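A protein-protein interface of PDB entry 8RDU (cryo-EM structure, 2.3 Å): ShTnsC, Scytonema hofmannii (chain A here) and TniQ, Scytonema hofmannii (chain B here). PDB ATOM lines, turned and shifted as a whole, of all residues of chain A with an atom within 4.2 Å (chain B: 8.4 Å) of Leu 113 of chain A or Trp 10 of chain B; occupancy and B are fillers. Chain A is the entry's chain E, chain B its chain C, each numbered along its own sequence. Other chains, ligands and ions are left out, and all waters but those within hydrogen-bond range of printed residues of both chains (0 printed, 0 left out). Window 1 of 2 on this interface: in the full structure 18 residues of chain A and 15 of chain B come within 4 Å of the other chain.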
ATOM      1  N   GLN A  81      -3.784  -4.334   8.994  1.00  0.00           N
ATOM      2  CA  GLN A  81      -4.540  -3.625   7.969  1.00  0.00           C
ATOM      3  C   GLN A  81      -4.375  -2.118   8.105  1.00  0.00           C
ATOM      4  O   GLN A  81      -4.226  -1.584   9.207  1.00  0.00           O
ATOM      5  CB  GLN A  81      -6.038  -3.969   8.053  1.00  0.00           C
ATOM      6  CG  GLN A  81      -6.879  -3.445   6.893  1.00  0.00           C
ATOM      7  CD  GLN A  81      -8.335  -3.854   6.988  1.00  0.00           C
ATOM      8  OE1 GLN A  81      -8.831  -4.176   8.065  1.00  0.00           O
ATOM      9  NE2 GLN A  81      -9.029  -3.829   5.861  1.00  0.00           N
ATOM     10  N   PRO A  86      -6.704  -3.635   1.332  1.00  0.00           N
ATOM     11  CA  PRO A  86      -6.901  -5.027   1.732  1.00  0.00           C
ATOM     12  C   PRO A  86      -6.024  -5.376   2.923  1.00  0.00           C
ATOM     13  O   PRO A  86      -4.878  -4.912   3.017  1.00  0.00           O
ATOM     14  CB  PRO A  86      -6.496  -5.817   0.478  1.00  0.00           C
ATOM     15  CG  PRO A  86      -5.535  -4.938  -0.218  1.00  0.00           C
ATOM     16  CD  PRO A  86      -6.006  -3.529   0.040  1.00  0.00           C
ATOM     17  N   PRO A  87      -6.524  -6.191   3.850  1.00  0.00           N
ATOM     18  CA  PRO A  87      -5.708  -6.586   5.003  1.00  0.00           C
ATOM     19  C   PRO A  87      -4.622  -7.571   4.598  1.00  0.00           C
ATOM     20  O   PRO A  87      -4.836  -8.436   3.749  1.00  0.00           O
ATOM     21  CB  PRO A  87      -6.728  -7.228   5.947  1.00  0.00           C
ATOM     22  CG  PRO A  87      -7.753  -7.798   5.027  1.00  0.00           C
ATOM     23  CD  PRO A  87      -7.856  -6.817   3.880  1.00  0.00           C
ATOM     24  N   VAL A  89      -3.106 -10.787   5.502  1.00  0.00           N
ATOM     25  CA  VAL A  89      -3.599 -11.936   6.259  1.00  0.00           C
ATOM     26  C   VAL A  89      -2.802 -13.174   5.870  1.00  0.00           C
ATOM     27  O   VAL A  89      -3.180 -13.878   4.924  1.00  0.00           O
ATOM     28  CB  VAL A  89      -5.105 -12.153   6.032  1.00  0.00           C
ATOM     29  CG1 VAL A  89      -5.628 -13.253   6.930  1.00  0.00           C
ATOM     30  CG2 VAL A  89      -5.880 -10.871   6.263  1.00  0.00           C
ATOM     31  N   VAL A  92      -5.112 -17.989   6.212  1.00  0.00           N
ATOM     32  CA  VAL A  92      -6.561 -18.110   6.107  1.00  0.00           C
ATOM     33  C   VAL A  92      -6.969 -19.474   6.646  1.00  0.00           C
ATOM     34  O   VAL A  92      -6.343 -20.489   6.321  1.00  0.00           O
ATOM     35  CB  VAL A  92      -7.033 -17.925   4.653  1.00  0.00           C
ATOM     36  CG1 VAL A  92      -8.522 -18.198   4.530  1.00  0.00           C
ATOM     37  CG2 VAL A  92      -6.716 -16.531   4.166  1.00  0.00           C
ATOM     38  N   ILE A 109     -13.793 -18.335   1.666  1.00  0.00           N
ATOM     39  CA  ILE A 109     -12.519 -17.615   1.628  1.00  0.00           C
ATOM     40  C   ILE A 109     -12.725 -16.102   1.659  1.00  0.00           C
ATOM     41  O   ILE A 109     -12.099 -15.397   2.459  1.00  0.00           O
ATOM     42  CB  ILE A 109     -11.692 -18.053   0.407  1.00  0.00           C
ATOM     43  CG1 ILE A 109     -11.269 -19.512   0.560  1.00  0.00           C
ATOM     44  CG2 ILE A 109     -10.469 -17.176   0.247  1.00  0.00           C
ATOM     45  CD1 ILE A 109     -10.682 -20.109  -0.676  1.00  0.00           C
ATOM     46  N   THR A 110     -13.584 -15.573   0.787  1.00  0.00           N
ATOM     47  CA  THR A 110     -13.802 -14.126   0.747  1.00  0.00           C
ATOM     48  C   THR A 110     -14.524 -13.599   1.985  1.00  0.00           C
ATOM     49  O   THR A 110     -14.308 -12.449   2.375  1.00  0.00           O
ATOM     50  CB  THR A 110     -14.585 -13.730  -0.510  1.00  0.00           C
ATOM     51  OG1 THR A 110     -15.789 -14.497  -0.593  1.00  0.00           O
ATOM     52  CG2 THR A 110     -13.765 -13.972  -1.754  1.00  0.00           C
ATOM     53  N   GLU A 111     -15.380 -14.406   2.613  1.00  0.00           N
ATOM     54  CA  GLU A 111     -15.979 -13.994   3.881  1.00  0.00           C
ATOM     55  C   GLU A 111     -14.973 -13.999   5.030  1.00  0.00           C
ATOM     56  O   GLU A 111     -15.058 -13.155   5.930  1.00  0.00           O
ATOM     57  CB  GLU A 111     -17.186 -14.874   4.206  1.00  0.00           C
ATOM     58  CG  GLU A 111     -18.390 -14.611   3.305  1.00  0.00           C
ATOM     59  CD  GLU A 111     -19.460 -15.684   3.412  1.00  0.00           C
ATOM     60  OE1 GLU A 111     -19.427 -16.469   4.382  1.00  0.00           O
ATOM     61  OE2 GLU A 111     -20.344 -15.739   2.533  1.00  0.00           O
ATOM     62  N   TYR A 112     -14.027 -14.940   5.036  1.00  0.00           N
ATOM     63  CA  TYR A 112     -12.977 -14.897   6.050  1.00  0.00           C
ATOM     64  C   TYR A 112     -12.164 -13.615   5.939  1.00  0.00           C
ATOM     65  O   TYR A 112     -11.848 -12.980   6.951  1.00  0.00           O
ATOM     66  CB  TYR A 112     -12.072 -16.121   5.934  1.00  0.00           C
ATOM     67  CG  TYR A 112     -11.026 -16.212   7.022  1.00  0.00           C
ATOM     68  CD1 TYR A 112     -11.295 -16.873   8.207  1.00  0.00           C
ATOM     69  CD2 TYR A 112      -9.767 -15.660   6.855  1.00  0.00           C
ATOM     70  CE1 TYR A 112     -10.354 -16.951   9.207  1.00  0.00           C
ATOM     71  CE2 TYR A 112      -8.818 -15.745   7.844  1.00  0.00           C
ATOM     72  CZ  TYR A 112      -9.116 -16.388   9.017  1.00  0.00           C
ATOM     73  OH  TYR A 112      -8.159 -16.492   9.996  1.00  0.00           O
ATOM     74  N   LEU A 113     -11.809 -13.224   4.721  1.00  0.00           N
ATOM     75  CA  LEU A 113     -11.079 -11.990   4.476  1.00  0.00           C
ATOM     76  C   LEU A 113     -11.975 -10.755   4.539  1.00  0.00           C
ATOM     77  O   LEU A 113     -11.480  -9.641   4.343  1.00  0.00           O
ATOM     78  CB  LEU A 113     -10.348 -12.089   3.133  1.00  0.00           C
ATOM     79  CG  LEU A 113      -9.272 -13.184   3.187  1.00  0.00           C
ATOM     80  CD1 LEU A 113      -8.705 -13.533   1.831  1.00  0.00           C
ATOM     81  CD2 LEU A 113      -8.155 -12.793   4.120  1.00  0.00           C
ATOM     82  N   LYS A 114     -13.267 -10.932   4.830  1.00  0.00           N
ATOM     83  CA  LYS A 114     -14.255  -9.851   4.917  1.00  0.00           C
ATOM     84  C   LYS A 114     -14.360  -9.013   3.644  1.00  0.00           C
ATOM     85  O   LYS A 114     -14.654  -7.818   3.703  1.00  0.00           O
ATOM     86  CB  LYS A 114     -13.964  -8.943   6.114  1.00  0.00           C
ATOM     87  CG  LYS A 114     -14.034  -9.646   7.453  1.00  0.00           C
ATOM     88  CD  LYS A 114     -13.841  -8.661   8.578  1.00  0.00           C
ATOM     89  CE  LYS A 114     -13.837  -9.343   9.937  1.00  0.00           C
ATOM     90  NZ  LYS A 114     -15.199  -9.782  10.343  1.00  0.00           N
ATOM     91  N   TYR A 115     -14.122  -9.620   2.486  1.00  0.00           N
ATOM     92  CA  TYR A 115     -14.364  -8.938   1.221  1.00  0.00           C
ATOM     93  C   TYR A 115     -15.868  -8.807   0.984  1.00  0.00           C
ATOM     94  O   TYR A 115     -16.616  -9.779   1.120  1.00  0.00           O
ATOM     95  CB  TYR A 115     -13.679  -9.706   0.095  1.00  0.00           C
ATOM     96  CG  TYR A 115     -13.823  -9.104  -1.275  1.00  0.00           C
ATOM     97  CD1 TYR A 115     -13.127  -7.961  -1.622  1.00  0.00           C
ATOM     98  CD2 TYR A 115     -14.617  -9.705  -2.235  1.00  0.00           C
ATOM     99  CE1 TYR A 115     -13.234  -7.422  -2.877  1.00  0.00           C
ATOM    100  CE2 TYR A 115     -14.729  -9.171  -3.495  1.00  0.00           C
ATOM    101  CZ  TYR A 115     -14.034  -8.029  -3.811  1.00  0.00           C
ATOM    102  OH  TYR A 115     -14.151  -7.484  -5.064  1.00  0.00           O
ATOM    103  N   ARG A 116     -16.308  -7.593   0.637  1.00  0.00           N
ATOM    104  CA  ARG A 116     -17.721  -7.225   0.724  1.00  0.00           C
ATOM    105  C   ARG A 116     -18.619  -7.800  -0.372  1.00  0.00           C
ATOM    106  O   ARG A 116     -19.842  -7.789  -0.198  1.00  0.00           O
ATOM    107  CB  ARG A 116     -17.862  -5.703   0.721  1.00  0.00           C
ATOM    108  CG  ARG A 116     -17.584  -5.064   2.064  1.00  0.00           C
ATOM    109  CD  ARG A 116     -17.350  -3.573   1.933  1.00  0.00           C
ATOM    110  NE  ARG A 116     -18.548  -2.881   1.472  1.00  0.00           N
ATOM    111  CZ  ARG A 116     -18.607  -1.586   1.203  1.00  0.00           C
ATOM    112  NH1 ARG A 116     -17.540  -0.809   1.301  1.00  0.00           N
ATOM    113  NH2 ARG A 116     -19.766  -1.054   0.822  1.00  0.00           N
ATOM    114  N   VAL A 132      -8.563 -11.547  -4.431  1.00  0.00           N
ATOM    115  CA  VAL A 132      -8.539 -11.262  -2.998  1.00  0.00           C
ATOM    116  C   VAL A 132      -7.394 -11.995  -2.299  1.00  0.00           C
ATOM    117  O   VAL A 132      -6.677 -11.410  -1.479  1.00  0.00           O
ATOM    118  CB  VAL A 132      -9.901 -11.595  -2.368  1.00  0.00           C
ATOM    119  CG1 VAL A 132      -9.767 -11.747  -0.892  1.00  0.00           C
ATOM    120  CG2 VAL A 132     -10.897 -10.504  -2.680  1.00  0.00           C
ATOM    121  N   CYS A 136      -4.541  -9.770  -0.513  1.00  0.00           N
ATOM    122  CA  CYS A 136      -4.307  -9.886   0.922  1.00  0.00           C
ATOM    123  C   CYS A 136      -2.965 -10.514   1.282  1.00  0.00           C
ATOM    124  O   CYS A 136      -2.649 -10.603   2.471  1.00  0.00           O
ATOM    125  CB  CYS A 136      -5.437 -10.681   1.575  1.00  0.00           C
ATOM    126  SG  CYS A 136      -7.071  -9.943   1.399  1.00  0.00           S
ATOM    127  N   GLU B   3     -13.613 -15.651  11.045  1.00  0.00           N
ATOM    128  CA  GLU B   3     -13.214 -14.355  10.509  1.00  0.00           C
ATOM    129  C   GLU B   3     -11.709 -14.148  10.601  1.00  0.00           C
ATOM    130  O   GLU B   3     -11.037 -14.770  11.421  1.00  0.00           O
ATOM    131  CB  GLU B   3     -13.924 -13.221  11.249  1.00  0.00           C
ATOM    132  CG  GLU B   3     -13.441 -13.032  12.676  1.00  0.00           C
ATOM    133  CD  GLU B   3     -14.156 -11.908  13.390  1.00  0.00           C
ATOM    134  OE1 GLU B   3     -14.767 -11.063  12.703  1.00  0.00           O
ATOM    135  OE2 GLU B   3     -14.113 -11.872  14.636  1.00  0.00           O
ATOM    136  N   ALA B   4     -11.185 -13.278   9.757  1.00  0.00           N
ATOM    137  CA  ALA B   4      -9.887 -12.677  10.023  1.00  0.00           C
ATOM    138  C   ALA B   4     -10.006 -11.650  11.144  1.00  0.00           C
ATOM    139  O   ALA B   4     -10.799 -10.706  11.027  1.00  0.00           O
ATOM    140  CB  ALA B   4      -9.328 -12.034   8.759  1.00  0.00           C
ATOM    141  N   PRO B   5      -9.265 -11.797  12.239  1.00  0.00           N
ATOM    142  CA  PRO B   5      -9.458 -10.907  13.389  1.00  0.00           C
ATOM    143  C   PRO B   5      -8.880  -9.514  13.162  1.00  0.00           C
ATOM    144  O   PRO B   5      -7.805  -9.351  12.582  1.00  0.00           O
ATOM    145  CB  PRO B   5      -8.736 -11.636  14.528  1.00  0.00           C
ATOM    146  CG  PRO B   5      -7.712 -12.466  13.858  1.00  0.00           C
ATOM    147  CD  PRO B   5      -8.294 -12.865  12.523  1.00  0.00           C
ATOM    148  N   VAL B   7     -10.084  -7.204  11.140  1.00  0.00           N
ATOM    149  CA  VAL B   7     -10.200  -6.770   9.754  1.00  0.00           C
ATOM    150  C   VAL B   7     -11.510  -6.008   9.613  1.00  0.00           C
ATOM    151  O   VAL B   7     -12.529  -6.387  10.201  1.00  0.00           O
ATOM    152  CB  VAL B   7     -10.129  -7.949   8.764  1.00  0.00           C
ATOM    153  CG1 VAL B   7     -10.486  -7.494   7.365  1.00  0.00           C
ATOM    154  CG2 VAL B   7      -8.736  -8.536   8.762  1.00  0.00           C
ATOM    155  N   LYS B   8     -11.472  -4.917   8.862  1.00  0.00           N
ATOM    156  CA  LYS B   8     -12.633  -4.094   8.563  1.00  0.00           C
ATOM    157  C   LYS B   8     -13.221  -4.478   7.212  1.00  0.00           C
ATOM    158  O   LYS B   8     -12.470  -4.707   6.257  1.00  0.00           O
ATOM    159  CB  LYS B   8     -12.273  -2.606   8.555  1.00  0.00           C
ATOM    160  CG  LYS B   8     -11.981  -1.985   9.927  1.00  0.00           C
ATOM    161  CD  LYS B   8     -10.690  -2.505  10.555  1.00  0.00           C
ATOM    162  CE  LYS B   8     -10.303  -1.707  11.784  1.00  0.00           C
ATOM    163  NZ  LYS B   8      -9.037  -2.211  12.385  1.00  0.00           N
ATOM    164  N   PRO B   9     -14.545  -4.578   7.097  1.00  0.00           N
ATOM    165  CA  PRO B   9     -15.135  -5.033   5.831  1.00  0.00           C
ATOM    166  C   PRO B   9     -14.771  -4.072   4.711  1.00  0.00           C
ATOM    167  O   PRO B   9     -14.957  -2.860   4.820  1.00  0.00           O
ATOM    168  CB  PRO B   9     -16.641  -5.038   6.119  1.00  0.00           C
ATOM    169  CG  PRO B   9     -16.821  -4.095   7.255  1.00  0.00           C
ATOM    170  CD  PRO B   9     -15.571  -4.208   8.083  1.00  0.00           C
ATOM    171  N   TRP B  10     -14.257  -4.632   3.620  1.00  0.00           N
ATOM    172  CA  TRP B  10     -13.493  -3.865   2.652  1.00  0.00           C
ATOM    173  C   TRP B  10     -13.816  -4.294   1.231  1.00  0.00           C
ATOM    174  O   TRP B  10     -14.421  -5.339   0.983  1.00  0.00           O
ATOM    175  CB  TRP B  10     -11.993  -4.020   2.921  1.00  0.00           C
ATOM    176  CG  TRP B  10     -11.491  -5.391   2.569  1.00  0.00           C
ATOM    177  CD1 TRP B  10     -11.585  -6.506   3.344  1.00  0.00           C
ATOM    178  CD2 TRP B  10     -10.846  -5.804   1.358  1.00  0.00           C
ATOM    179  NE1 TRP B  10     -11.030  -7.580   2.706  1.00  0.00           N
ATOM    180  CE2 TRP B  10     -10.569  -7.179   1.482  1.00  0.00           C
ATOM    181  CE3 TRP B  10     -10.470  -5.145   0.187  1.00  0.00           C
ATOM    182  CZ2 TRP B  10      -9.938  -7.907   0.480  1.00  0.00           C
ATOM    183  CZ3 TRP B  10      -9.845  -5.870  -0.804  1.00  0.00           C
ATOM    184  CH2 TRP B  10      -9.582  -7.235  -0.652  1.00  0.00           C
ATOM    185  N   LEU B  11     -13.395  -3.444   0.297  1.00  0.00           N
ATOM    186  CA  LEU B  11     -13.663  -3.609  -1.118  1.00  0.00           C
ATOM    187  C   LEU B  11     -12.484  -3.015  -1.875  1.00  0.00           C
ATOM    188  O   LEU B  11     -11.809  -2.117  -1.366  1.00  0.00           O
ATOM    189  CB  LEU B  11     -14.976  -2.905  -1.477  1.00  0.00           C
ATOM    190  CG  LEU B  11     -15.653  -3.123  -2.814  1.00  0.00           C
ATOM    191  CD1 LEU B  11     -15.908  -4.590  -2.939  1.00  0.00           C
ATOM    192  CD2 LEU B  11     -16.958  -2.366  -2.842  1.00  0.00           C
ATOM    193  N   PHE B  12     -12.222  -3.514  -3.081  1.00  0.00           N
ATOM    194  CA  PHE B  12     -11.156  -2.915  -3.874  1.00  0.00           C
ATOM    195  C   PHE B  12     -11.578  -1.532  -4.353  1.00  0.00           C
ATOM    196  O   PHE B  12     -12.651  -1.365  -4.939  1.00  0.00           O
ATOM    197  CB  PHE B  12     -10.779  -3.798  -5.061  1.00  0.00           C
ATOM    198  CG  PHE B  12     -10.144  -5.099  -4.676  1.00  0.00           C
ATOM    199  CD1 PHE B  12      -8.857  -5.128  -4.166  1.00  0.00           C
ATOM    200  CD2 PHE B  12     -10.809  -6.296  -4.859  1.00  0.00           C
ATOM    201  CE1 PHE B  12      -8.259  -6.319  -3.819  1.00  0.00           C
ATOM    202  CE2 PHE B  12     -10.214  -7.492  -4.515  1.00  0.00           C
ATOM    203  CZ  PHE B  12      -8.935  -7.502  -3.996  1.00  0.00           C
ATOM    204  N   LEU B  13     -10.735  -0.543  -4.094  1.00  0.00           N
ATOM    205  CA  LEU B  13     -10.983   0.841  -4.465  1.00  0.00           C
ATOM    206  C   LEU B  13     -10.133   1.247  -5.661  1.00  0.00           C
ATOM    207  O   LEU B  13      -9.145   0.594  -6.004  1.00  0.00           O
ATOM    208  CB  LEU B  13     -10.706   1.768  -3.282  1.00  0.00           C
ATOM    209  CG  LEU B  13     -11.431   1.350  -2.005  1.00  0.00           C
ATOM    210  CD1 LEU B  13     -11.165   2.333  -0.887  1.00  0.00           C
ATOM    211  CD2 LEU B  13     -12.918   1.225  -2.275  1.00  0.00           C
ATOM    212  N   PHE B  29     -14.065   0.495 -11.579  1.00  0.00           N
ATOM    213  CA  PHE B  29     -14.472  -0.058 -10.290  1.00  0.00           C
ATOM    214  C   PHE B  29     -15.112  -1.431 -10.441  1.00  0.00           C
ATOM    215  O   PHE B  29     -14.887  -2.326  -9.621  1.00  0.00           O
ATOM    216  CB  PHE B  29     -15.436   0.894  -9.586  1.00  0.00           C
ATOM    217  CG  PHE B  29     -15.782   0.470  -8.188  1.00  0.00           C
ATOM    218  CD1 PHE B  29     -14.995   0.858  -7.120  1.00  0.00           C
ATOM    219  CD2 PHE B  29     -16.888  -0.324  -7.942  1.00  0.00           C
ATOM    220  CE1 PHE B  29     -15.302   0.465  -5.839  1.00  0.00           C
ATOM    221  CE2 PHE B  29     -17.199  -0.718  -6.661  1.00  0.00           C
ATOM    222  CZ  PHE B  29     -16.404  -0.321  -5.610  1.00  0.00           C
ATOM    223  N   ALA B  32     -12.237  -3.845 -11.277  1.00  0.00           N
ATOM    224  CA  ALA B  32     -11.469  -4.086 -10.058  1.00  0.00           C
ATOM    225  C   ALA B  32     -12.150  -5.063  -9.112  1.00  0.00           C
ATOM    226  O   ALA B  32     -11.470  -5.705  -8.307  1.00  0.00           O
ATOM    227  CB  ALA B  32     -11.209  -2.767  -9.332  1.00  0.00           C
ATOM    228  N   ASN B  33     -13.470  -5.195  -9.193  1.00  0.00           N
ATOM    229  CA  ASN B  33     -14.220  -6.100  -8.335  1.00  0.00           C
ATOM    230  C   ASN B  33     -14.940  -7.194  -9.110  1.00  0.00           C
ATOM    231  O   ASN B  33     -15.800  -7.866  -8.539  1.00  0.00           O
ATOM    232  CB  ASN B  33     -15.220  -5.313  -7.485  1.00  0.00           C
ATOM    233  CG  ASN B  33     -14.538  -4.379  -6.508  1.00  0.00           C
ATOM    234  OD1 ASN B  33     -13.994  -4.813  -5.497  1.00  0.00           O
ATOM    235  ND2 ASN B  33     -14.566  -3.089  -6.804  1.00  0.00           N
ATOM    236  N   VAL B  73     -20.866   2.472  -1.718  1.00  0.00           N
ATOM    237  CA  VAL B  73     -20.115   1.288  -2.107  1.00  0.00           C
ATOM    238  C   VAL B  73     -18.769   1.669  -2.709  1.00  0.00           C
ATOM    239  O   VAL B  73     -17.748   1.056  -2.402  1.00  0.00           O
ATOM    240  CB  VAL B  73     -20.945   0.394  -3.059  1.00  0.00           C
ATOM    241  CG1 VAL B  73     -22.297   0.090  -2.440  1.00  0.00           C
ATOM    242  CG2 VAL B  73     -21.149   1.038  -4.410  1.00  0.00           C
ATOM    243  N   GLU B  75     -16.015   4.455  -2.325  1.00  0.00           N
ATOM    244  CA  GLU B  75     -15.659   5.333  -1.220  1.00  0.00           C
ATOM    245  C   GLU B  75     -15.425   6.770  -1.661  1.00  0.00           C
ATOM    246  O   GLU B  75     -15.115   7.621  -0.821  1.00  0.00           O
ATOM    247  CB  GLU B  75     -14.410   4.795  -0.520  1.00  0.00           C
ATOM    248  CG  GLU B  75     -14.584   3.405   0.065  1.00  0.00           C
ATOM    249  CD  GLU B  75     -15.636   3.342   1.146  1.00  0.00           C
ATOM    250  OE1 GLU B  75     -15.837   4.357   1.846  1.00  0.00           O
ATOM    251  OE2 GLU B  75     -16.263   2.275   1.299  1.00  0.00           O
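Hydrophobic or aromatic side chains of chain B that line the printed part of chain A: Ala 4, Val 7, Trp 10, Leu 11 and Phe 12. Among the printed residues, 24 pairs touch across the chains.
Of the printed residues of chain B, Leu 113 of chain A touches Val 7 and Trp 10. Of the printed residues of chain B, Pro 87 of chain A touches Val 7 and Trp 10. Printed residues of chain A within 4 Å of Phe 12 of chain B: Tyr 115 (3.3 Å) and Val 132 (3.6 Å). Of the printed residues of chain B, Lys 114 of chain A touches Glu 3 (2.7 Å), Ala 4 (3.5 Å), Val 7 (3.1 Å), Pro 9 (3.5 Å) and Trp 10 (3.2 Å). Val 92 of chain A touches none of the printed residues of chain B. The nearest residue of chain B that does not touch Leu 113 of chain A is Ala 4 of chain B (4.6 Å).
Among the printed residues, merely in contact across the chains: Lys 114 of chain A with Val 7 of chain B, Tyr 112 of chain A with Glu 3 of chain B, Tyr 115 of chain A with Phe 12 of chain B, Gln 81 of chain A with Val 7 of chain B, Pro 87 of chain A with Trp 10 of chain B, Lys 114 of chain A with Ala 4 of chain B, Lys 114 of chain A with Pro 9 of chain B, Pro 86 of chain A with Trp 10 of chain B, Val 132 of chain A with Phe 12 of chain B, Tyr 115 of chain A with Trp 10 of chain B, Pro 87 of chain A with Val 7 of chain B, Cys 136 of chain A with Trp 10 of chain B, Arg 116 of chain A with Val 73 of chain B, Arg 116 of chain A with Pro 9 of chain B, Leu 113 of chain A with Val 7 of chain B and Tyr 115 of chain A with Leu 11 of chain B.
O of Val 132 of chain A sits at hydrogen-bond distance from SG of Cys 136 of chain A (3.3 Å). The backbone carbonyl oxygen (O) of Thr 110 of chain A is in hydrogen-bond range of the backbone NH (N) of Tyr 115 of chain A, 2.8 Å away. N of Val 89 of chain A lies within hydrogen-bond range of O of Cys 136 of chain A, at 3.1 Å. O of Phe 12 of chain B is in hydrogen-bond range of ND2 of Asn 33 of chain B, at 3.2 Å. The backbone carbonyl oxygen (O) of Phe 29 of chain B sits at hydrogen-bond distance from the side-chain amide nitrogen (ND2) of Asn 33 of chain B (2.9 Å). The backbone carbonyl oxygen (O) of Pro 87 of chain A lies close to the side-chain sulfur (SG) of Cys 136 of chain A (3.6 Å).
The side-chain carboxylate of Glu 75 of chain B is in salt-bridge range of the guanidinium group of Arg 116 of chain A (3.3 Å). The backbone carbonyl oxygen of Trp 10 of chain B is in hydrogen-bond range of the backbone NH of Arg 116 of chain A, 3.0 Å away. O of Leu 113 of chain A is in hydrogen-bond range of NE1 of Trp 10 of chain B (2.7 Å). The side-chain amide oxygen (OD1) of Asn 33 of chain B lies within hydrogen-bond range of the side-chain hydroxyl (OH) of Tyr 115 of chain A. N of Trp 10 of chain B is in hydrogen-bond range of O of Lys 114 of chain A, 3.2 Å away. The backbone NH (N) of Ala 4 of chain B sits at hydrogen-bond distance from the backbone carbonyl oxygen (O) of Tyr 112 of chain A (2.9 Å). The side-chain carboxylate (OE1) of Glu 3 of chain B is in salt-bridge range of the side-chain amino group (NZ) of Lys 114 of chain A (2.7 Å). N of Lys 8 of chain B sits at hydrogen-bond distance from OE1 of Gln 81 of chain A (2.9 Å).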
